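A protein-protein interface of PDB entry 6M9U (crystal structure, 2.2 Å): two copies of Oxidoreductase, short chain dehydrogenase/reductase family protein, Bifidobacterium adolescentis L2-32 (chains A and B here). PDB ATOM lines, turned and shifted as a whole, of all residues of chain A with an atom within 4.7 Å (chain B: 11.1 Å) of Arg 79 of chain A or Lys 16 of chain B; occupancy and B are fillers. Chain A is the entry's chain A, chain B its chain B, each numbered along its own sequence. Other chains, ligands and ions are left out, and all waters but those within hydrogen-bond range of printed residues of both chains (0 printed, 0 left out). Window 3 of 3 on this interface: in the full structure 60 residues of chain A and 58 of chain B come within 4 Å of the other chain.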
ATOM      1  N   ASP A  75     -25.056 -29.807 -19.249  1.00  0.00           N
ATOM      2  CA  ASP A  75     -24.779 -28.773 -18.265  1.00  0.00           C
ATOM      3  C   ASP A  75     -24.238 -27.503 -18.893  1.00  0.00           C
ATOM      4  O   ASP A  75     -24.576 -26.403 -18.450  1.00  0.00           O
ATOM      5  CB  ASP A  75     -23.756 -29.272 -17.247  1.00  0.00           C
ATOM      6  CG  ASP A  75     -24.310 -30.259 -16.281  1.00  0.00           C
ATOM      7  OD1 ASP A  75     -25.537 -30.271 -16.068  1.00  0.00           O
ATOM      8  OD2 ASP A  75     -23.491 -31.003 -15.706  1.00  0.00           O
ATOM      9  N   MET A  76     -23.343 -27.618 -19.880  1.00  0.00           N
ATOM     10  CA  MET A  76     -22.694 -26.470 -20.486  1.00  0.00           C
ATOM     11  C   MET A  76     -23.505 -25.879 -21.615  1.00  0.00           C
ATOM     12  O   MET A  76     -23.469 -24.665 -21.819  1.00  0.00           O
ATOM     13  CB  MET A  76     -21.328 -26.827 -21.072  1.00  0.00           C
ATOM     14  CG  MET A  76     -20.353 -27.280 -20.062  1.00  0.00           C
ATOM     15  SD  MET A  76     -18.813 -27.581 -20.927  1.00  0.00           S
ATOM     16  CE  MET A  76     -18.025 -28.477 -19.668  1.00  0.00           C
ATOM     17  N   SER A  77     -24.187 -26.722 -22.397  1.00  0.00           N
ATOM     18  CA  SER A  77     -25.117 -26.185 -23.387  1.00  0.00           C
ATOM     19  C   SER A  77     -26.165 -25.317 -22.703  1.00  0.00           C
ATOM     20  O   SER A  77     -26.493 -24.219 -23.182  1.00  0.00           O
ATOM     21  CB  SER A  77     -25.814 -27.314 -24.140  1.00  0.00           C
ATOM     22  OG  SER A  77     -24.885 -28.022 -24.917  1.00  0.00           O
ATOM     23  N   GLU A  78     -26.668 -25.779 -21.551  1.00  0.00           N
ATOM     24  CA  GLU A  78     -27.722 -25.045 -20.868  1.00  0.00           C
ATOM     25  C   GLU A  78     -27.205 -23.731 -20.305  1.00  0.00           C
ATOM     26  O   GLU A  78     -27.825 -22.670 -20.496  1.00  0.00           O
ATOM     27  CB  GLU A  78     -28.311 -25.909 -19.772  1.00  0.00           C
ATOM     28  CG  GLU A  78     -29.195 -27.007 -20.316  1.00  0.00           C
ATOM     29  CD  GLU A  78     -29.717 -27.957 -19.247  1.00  0.00           C
ATOM     30  OE1 GLU A  78     -29.296 -27.867 -18.059  1.00  0.00           O
ATOM     31  OE2 GLU A  78     -30.566 -28.795 -19.614  1.00  0.00           O
ATOM     32  N   ARG A  79     -26.080 -23.790 -19.596  1.00  0.00           N
ATOM     33  CA  ARG A  79     -25.546 -22.610 -18.945  1.00  0.00           C
ATOM     34  C   ARG A  79     -25.087 -21.527 -19.916  1.00  0.00           C
ATOM     35  O   ARG A  79     -25.228 -20.333 -19.618  1.00  0.00           O
ATOM     36  CB  ARG A  79     -24.385 -23.025 -18.049  1.00  0.00           C
ATOM     37  CG  ARG A  79     -24.823 -23.765 -16.814  1.00  0.00           C
ATOM     38  CD  ARG A  79     -23.622 -23.995 -15.964  1.00  0.00           C
ATOM     39  NE  ARG A  79     -23.946 -24.423 -14.627  1.00  0.00           N
ATOM     40  CZ  ARG A  79     -24.467 -25.585 -14.318  1.00  0.00           C
ATOM     41  NH1 ARG A  79     -24.759 -26.474 -15.262  1.00  0.00           N
ATOM     42  NH2 ARG A  79     -24.679 -25.858 -13.037  1.00  0.00           N
ATOM     43  N   PHE A  80     -24.514 -21.893 -21.057  1.00  0.00           N
ATOM     44  CA  PHE A  80     -23.828 -20.900 -21.874  1.00  0.00           C
ATOM     45  C   PHE A  80     -24.394 -20.719 -23.267  1.00  0.00           C
ATOM     46  O   PHE A  80     -23.893 -19.878 -24.013  1.00  0.00           O
ATOM     47  CB  PHE A  80     -22.332 -21.280 -21.981  1.00  0.00           C
ATOM     48  CG  PHE A  80     -21.692 -21.594 -20.658  1.00  0.00           C
ATOM     49  CD1 PHE A  80     -21.728 -20.664 -19.630  1.00  0.00           C
ATOM     50  CD2 PHE A  80     -21.127 -22.811 -20.426  1.00  0.00           C
ATOM     51  CE1 PHE A  80     -21.160 -20.960 -18.396  1.00  0.00           C
ATOM     52  CE2 PHE A  80     -20.579 -23.108 -19.195  1.00  0.00           C
ATOM     53  CZ  PHE A  80     -20.562 -22.202 -18.207  1.00  0.00           C
ATOM     54  N   GLY A  81     -25.393 -21.488 -23.659  1.00  0.00           N
ATOM     55  CA  GLY A  81     -26.061 -21.150 -24.903  1.00  0.00           C
ATOM     56  C   GLY A  81     -25.328 -21.444 -26.191  1.00  0.00           C
ATOM     57  O   GLY A  81     -25.773 -20.983 -27.249  1.00  0.00           O
ATOM     58  N   TYR B  10     -11.487 -24.841  -2.506  1.00  0.00           N
ATOM     59  CA  TYR B  10     -10.982 -25.400  -3.756  1.00  0.00           C
ATOM     60  C   TYR B  10     -12.121 -26.008  -4.557  1.00  0.00           C
ATOM     61  O   TYR B  10     -12.181 -27.224  -4.771  1.00  0.00           O
ATOM     62  CB  TYR B  10      -9.911 -26.462  -3.496  1.00  0.00           C
ATOM     63  CG  TYR B  10      -8.634 -25.994  -2.841  1.00  0.00           C
ATOM     64  CD1 TYR B  10      -7.941 -24.889  -3.314  1.00  0.00           C
ATOM     65  CD2 TYR B  10      -8.117 -26.680  -1.757  1.00  0.00           C
ATOM     66  CE1 TYR B  10      -6.780 -24.489  -2.728  1.00  0.00           C
ATOM     67  CE2 TYR B  10      -6.965 -26.283  -1.158  1.00  0.00           C
ATOM     68  CZ  TYR B  10      -6.290 -25.187  -1.657  1.00  0.00           C
ATOM     69  OH  TYR B  10      -5.120 -24.788  -1.074  1.00  0.00           O
ATOM     70  N   PRO B  11     -13.012 -25.187  -5.077  1.00  0.00           N
ATOM     71  CA  PRO B  11     -14.014 -25.718  -5.998  1.00  0.00           C
ATOM     72  C   PRO B  11     -13.333 -26.457  -7.142  1.00  0.00           C
ATOM     73  O   PRO B  11     -12.261 -26.071  -7.621  1.00  0.00           O
ATOM     74  CB  PRO B  11     -14.752 -24.471  -6.490  1.00  0.00           C
ATOM     75  CG  PRO B  11     -14.291 -23.369  -5.630  1.00  0.00           C
ATOM     76  CD  PRO B  11     -12.958 -23.724  -5.088  1.00  0.00           C
ATOM     77  N   LEU B  12     -13.975 -27.523  -7.595  1.00  0.00           N
ATOM     78  CA  LEU B  12     -13.531 -28.258  -8.768  1.00  0.00           C
ATOM     79  C   LEU B  12     -14.135 -27.728 -10.043  1.00  0.00           C
ATOM     80  O   LEU B  12     -13.571 -27.937 -11.118  1.00  0.00           O
ATOM     81  CB  LEU B  12     -13.907 -29.726  -8.629  1.00  0.00           C
ATOM     82  CG  LEU B  12     -13.418 -30.407  -7.351  1.00  0.00           C
ATOM     83  CD1 LEU B  12     -13.800 -31.856  -7.444  1.00  0.00           C
ATOM     84  CD2 LEU B  12     -11.938 -30.249  -7.196  1.00  0.00           C
ATOM     85  N   ASP B  13     -15.277 -27.020  -9.943  1.00  0.00           N
ATOM     86  CA  ASP B  13     -16.083 -26.669 -11.113  1.00  0.00           C
ATOM     87  C   ASP B  13     -16.791 -25.342 -10.863  1.00  0.00           C
ATOM     88  O   ASP B  13     -18.018 -25.271 -10.763  1.00  0.00           O
ATOM     89  CB  ASP B  13     -17.080 -27.796 -11.396  1.00  0.00           C
ATOM     90  CG  ASP B  13     -16.390 -29.108 -11.798  1.00  0.00           C
ATOM     91  OD1 ASP B  13     -15.930 -29.137 -12.959  1.00  0.00           O
ATOM     92  OD2 ASP B  13     -16.289 -30.049 -10.976  1.00  0.00           O
ATOM     93  N   LYS B  14     -16.002 -24.270 -10.781  1.00  0.00           N
ATOM     94  CA  LYS B  14     -16.578 -22.954 -10.528  1.00  0.00           C
ATOM     95  C   LYS B  14     -17.630 -22.622 -11.583  1.00  0.00           C
ATOM     96  O   LYS B  14     -18.643 -21.972 -11.290  1.00  0.00           O
ATOM     97  CB  LYS B  14     -15.494 -21.880 -10.514  1.00  0.00           C
ATOM     98  CG  LYS B  14     -14.628 -21.865  -9.279  1.00  0.00           C
ATOM     99  CD  LYS B  14     -13.802 -20.573  -9.282  1.00  0.00           C
ATOM    100  CE  LYS B  14     -12.846 -20.506  -8.103  1.00  0.00           C
ATOM    101  NZ  LYS B  14     -11.717 -19.577  -8.432  1.00  0.00           N
ATOM    102  N   TRP B  15     -17.395 -23.072 -12.830  1.00  0.00           N
ATOM    103  CA  TRP B  15     -18.279 -22.755 -13.947  1.00  0.00           C
ATOM    104  C   TRP B  15     -19.698 -23.266 -13.720  1.00  0.00           C
ATOM    105  O   TRP B  15     -20.613 -22.920 -14.477  1.00  0.00           O
ATOM    106  CB  TRP B  15     -17.730 -23.390 -15.237  1.00  0.00           C
ATOM    107  CG  TRP B  15     -17.667 -24.947 -15.129  1.00  0.00           C
ATOM    108  CD1 TRP B  15     -16.647 -25.709 -14.593  1.00  0.00           C
ATOM    109  CD2 TRP B  15     -18.678 -25.882 -15.529  1.00  0.00           C
ATOM    110  NE1 TRP B  15     -16.957 -27.049 -14.661  1.00  0.00           N
ATOM    111  CE2 TRP B  15     -18.203 -27.183 -15.225  1.00  0.00           C
ATOM    112  CE3 TRP B  15     -19.924 -25.750 -16.146  1.00  0.00           C
ATOM    113  CZ2 TRP B  15     -18.952 -28.327 -15.489  1.00  0.00           C
ATOM    114  CZ3 TRP B  15     -20.645 -26.902 -16.419  1.00  0.00           C
ATOM    115  CH2 TRP B  15     -20.150 -28.161 -16.089  1.00  0.00           C
ATOM    116  N   LYS B  16     -19.885 -24.141 -12.736  1.00  0.00           N
ATOM    117  CA  LYS B  16     -21.241 -24.620 -12.419  1.00  0.00           C
ATOM    118  C   LYS B  16     -22.074 -23.573 -11.729  1.00  0.00           C
ATOM    119  O   LYS B  16     -23.307 -23.607 -11.829  1.00  0.00           O
ATOM    120  CB  LYS B  16     -21.162 -25.855 -11.541  1.00  0.00           C
ATOM    121  CG  LYS B  16     -20.879 -27.103 -12.374  1.00  0.00           C
ATOM    122  CD  LYS B  16     -20.876 -28.311 -11.500  1.00  0.00           C
ATOM    123  CE  LYS B  16     -20.890 -29.567 -12.351  1.00  0.00           C
ATOM    124  NZ  LYS B  16     -20.777 -30.730 -11.454  1.00  0.00           N
ATOM    125  N   ASP B  17     -21.425 -22.649 -11.025  1.00  0.00           N
ATOM    126  CA  ASP B  17     -22.084 -21.568 -10.282  1.00  0.00           C
ATOM    127  C   ASP B  17     -22.523 -20.430 -11.199  1.00  0.00           C
ATOM    128  O   ASP B  17     -21.726 -19.942 -12.004  1.00  0.00           O
ATOM    129  CB  ASP B  17     -21.092 -21.078  -9.243  1.00  0.00           C
ATOM    130  CG  ASP B  17     -21.666 -20.092  -8.316  1.00  0.00           C
ATOM    131  OD1 ASP B  17     -22.406 -19.194  -8.783  1.00  0.00           O
ATOM    132  OD2 ASP B  17     -21.358 -20.237  -7.110  1.00  0.00           O
ATOM    133  N   SER B  18     -23.793 -20.025 -11.102  1.00  0.00           N
ATOM    134  CA  SER B  18     -24.318 -19.032 -12.030  1.00  0.00           C
ATOM    135  C   SER B  18     -23.597 -17.705 -11.886  1.00  0.00           C
ATOM    136  O   SER B  18     -23.510 -16.928 -12.841  1.00  0.00           O
ATOM    137  CB  SER B  18     -25.807 -18.764 -11.827  1.00  0.00           C
ATOM    138  OG  SER B  18     -26.594 -19.660 -12.566  1.00  0.00           O
ATOM    139  N   ASN B  19     -23.079 -17.417 -10.708  1.00  0.00           N
ATOM    140  CA  ASN B  19     -22.320 -16.192 -10.490  1.00  0.00           C
ATOM    141  C   ASN B  19     -20.896 -16.205 -11.056  1.00  0.00           C
ATOM    142  O   ASN B  19     -20.256 -15.152 -11.076  1.00  0.00           O
ATOM    143  CB  ASN B  19     -22.259 -15.910  -8.985  1.00  0.00           C
ATOM    144  CG  ASN B  19     -22.050 -14.444  -8.681  1.00  0.00           C
ATOM    145  OD1 ASN B  19     -22.552 -13.562  -9.389  1.00  0.00           O
ATOM    146  ND2 ASN B  19     -21.292 -14.172  -7.633  1.00  0.00           N
ATOM    147  N   TYR B  20     -20.370 -17.343 -11.498  1.00  0.00           N
ATOM    148  CA  TYR B  20     -19.060 -17.361 -12.113  1.00  0.00           C
ATOM    149  C   TYR B  20     -19.190 -16.879 -13.544  1.00  0.00           C
ATOM    150  O   TYR B  20     -20.148 -17.213 -14.235  1.00  0.00           O
ATOM    151  CB  TYR B  20     -18.472 -18.763 -12.096  1.00  0.00           C
ATOM    152  CG  TYR B  20     -17.094 -18.843 -12.703  1.00  0.00           C
ATOM    153  CD1 TYR B  20     -15.979 -18.531 -11.952  1.00  0.00           C
ATOM    154  CD2 TYR B  20     -16.924 -19.221 -14.027  1.00  0.00           C
ATOM    155  CE1 TYR B  20     -14.722 -18.577 -12.514  1.00  0.00           C
ATOM    156  CE2 TYR B  20     -15.698 -19.275 -14.588  1.00  0.00           C
ATOM    157  CZ  TYR B  20     -14.599 -18.965 -13.819  1.00  0.00           C
ATOM    158  OH  TYR B  20     -13.363 -19.042 -14.394  1.00  0.00           O
ATOM    159  N   SER B  21     -18.239 -16.060 -13.977  1.00  0.00           N
ATOM    160  CA  SER B  21     -18.193 -15.598 -15.362  1.00  0.00           C
ATOM    161  C   SER B  21     -16.733 -15.521 -15.789  1.00  0.00           C
ATOM    162  O   SER B  21     -15.962 -14.736 -15.235  1.00  0.00           O
ATOM    163  CB  SER B  21     -18.867 -14.238 -15.509  1.00  0.00           C
ATOM    164  OG  SER B  21     -18.622 -13.741 -16.794  1.00  0.00           O
ATOM    165  N   ILE B  22     -16.346 -16.317 -16.776  1.00  0.00           N
ATOM    166  CA  ILE B  22     -14.925 -16.418 -17.127  1.00  0.00           C
ATOM    167  C   ILE B  22     -14.423 -15.084 -17.642  1.00  0.00           C
ATOM    168  O   ILE B  22     -13.350 -14.606 -17.231  1.00  0.00           O
ATOM    169  CB  ILE B  22     -14.677 -17.557 -18.143  1.00  0.00           C
ATOM    170  CG1 ILE B  22     -13.163 -17.697 -18.418  1.00  0.00           C
ATOM    171  CG2 ILE B  22     -15.408 -17.324 -19.464  1.00  0.00           C
ATOM    172  CD1 ILE B  22     -12.385 -18.240 -17.233  1.00  0.00           C
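The backbone carbonyl oxygen of Lys 16 of chain B is in hydrogen-bond range of the guanidinium group of Arg 79 of chain A.
The side-chain carboxylate of Asp 75 of chain A lies within salt-bridge range of the guanidinium group of Arg 79 of chain A.
The side-chain carboxylate (OD1) of Asp 13 of chain B is in hydrogen-bond range of the indole nitrogen (NE1) of Trp 15 of chain B, 2.9 Å away.
Among the printed residues, merely in contact across the chains: Arg 79 of chain A with Trp 15 of chain B (3.5 Å), Met 76 of chain A with Trp 15 of chain B (3.7 Å), Phe 80 of chain A with Trp 15 of chain B (3.8 Å) and Asp 75 of chain A with Trp 15 of chain B (3.9 Å).
Of chain B, only Trp 15 comes within 4 Å of Asp 75 of chain A.
Of the printed residues of chain B, Met 76 of chain A touches Trp 15.
No residue of chain B comes within 4 Å of Ser 77 of chain A.
No residue of chain B comes within 4 Å of Glu 78 of chain A.
Arg 79 of chain A touches just these residues of chain B: Trp 15 (3.5 Å) and Lys 16 (2.9 Å).
Phe 80 of chain A touches one residue of chain B.
Printed residues of chain A within 4 Å of Trp 15 of chain B: Asp 75 (3.9 Å), Met 76 (3.7 Å), Arg 79 (3.5 Å) and Phe 80 (3.8 Å).
Lys 16 of chain B touches just one residue of chain A: Arg 79.
The nearest residue of chain B that does not touch Arg 79 of chain A is Asp 17 of chain B (4.7 Å).
The nearest printed residue of chain A that does not touch Trp 15 of chain B is Ser 77 of chain A (7.0 Å).
Of the 7 printed residues of chain A, 4 touch a printed residue of chain B.
Hydrophobic or aromatic side chains of chain B within 4 Å of the printed part of chain A: Trp 15.
Along chain B the printed residues that touch a printed residue of chain A span positions 15 to 16.
Among the printed residues, no Asp or Glu carboxylate lies within 4 Å of a Lys or Arg side-chain nitrogen of the other chain.
No position is printed for both chains.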
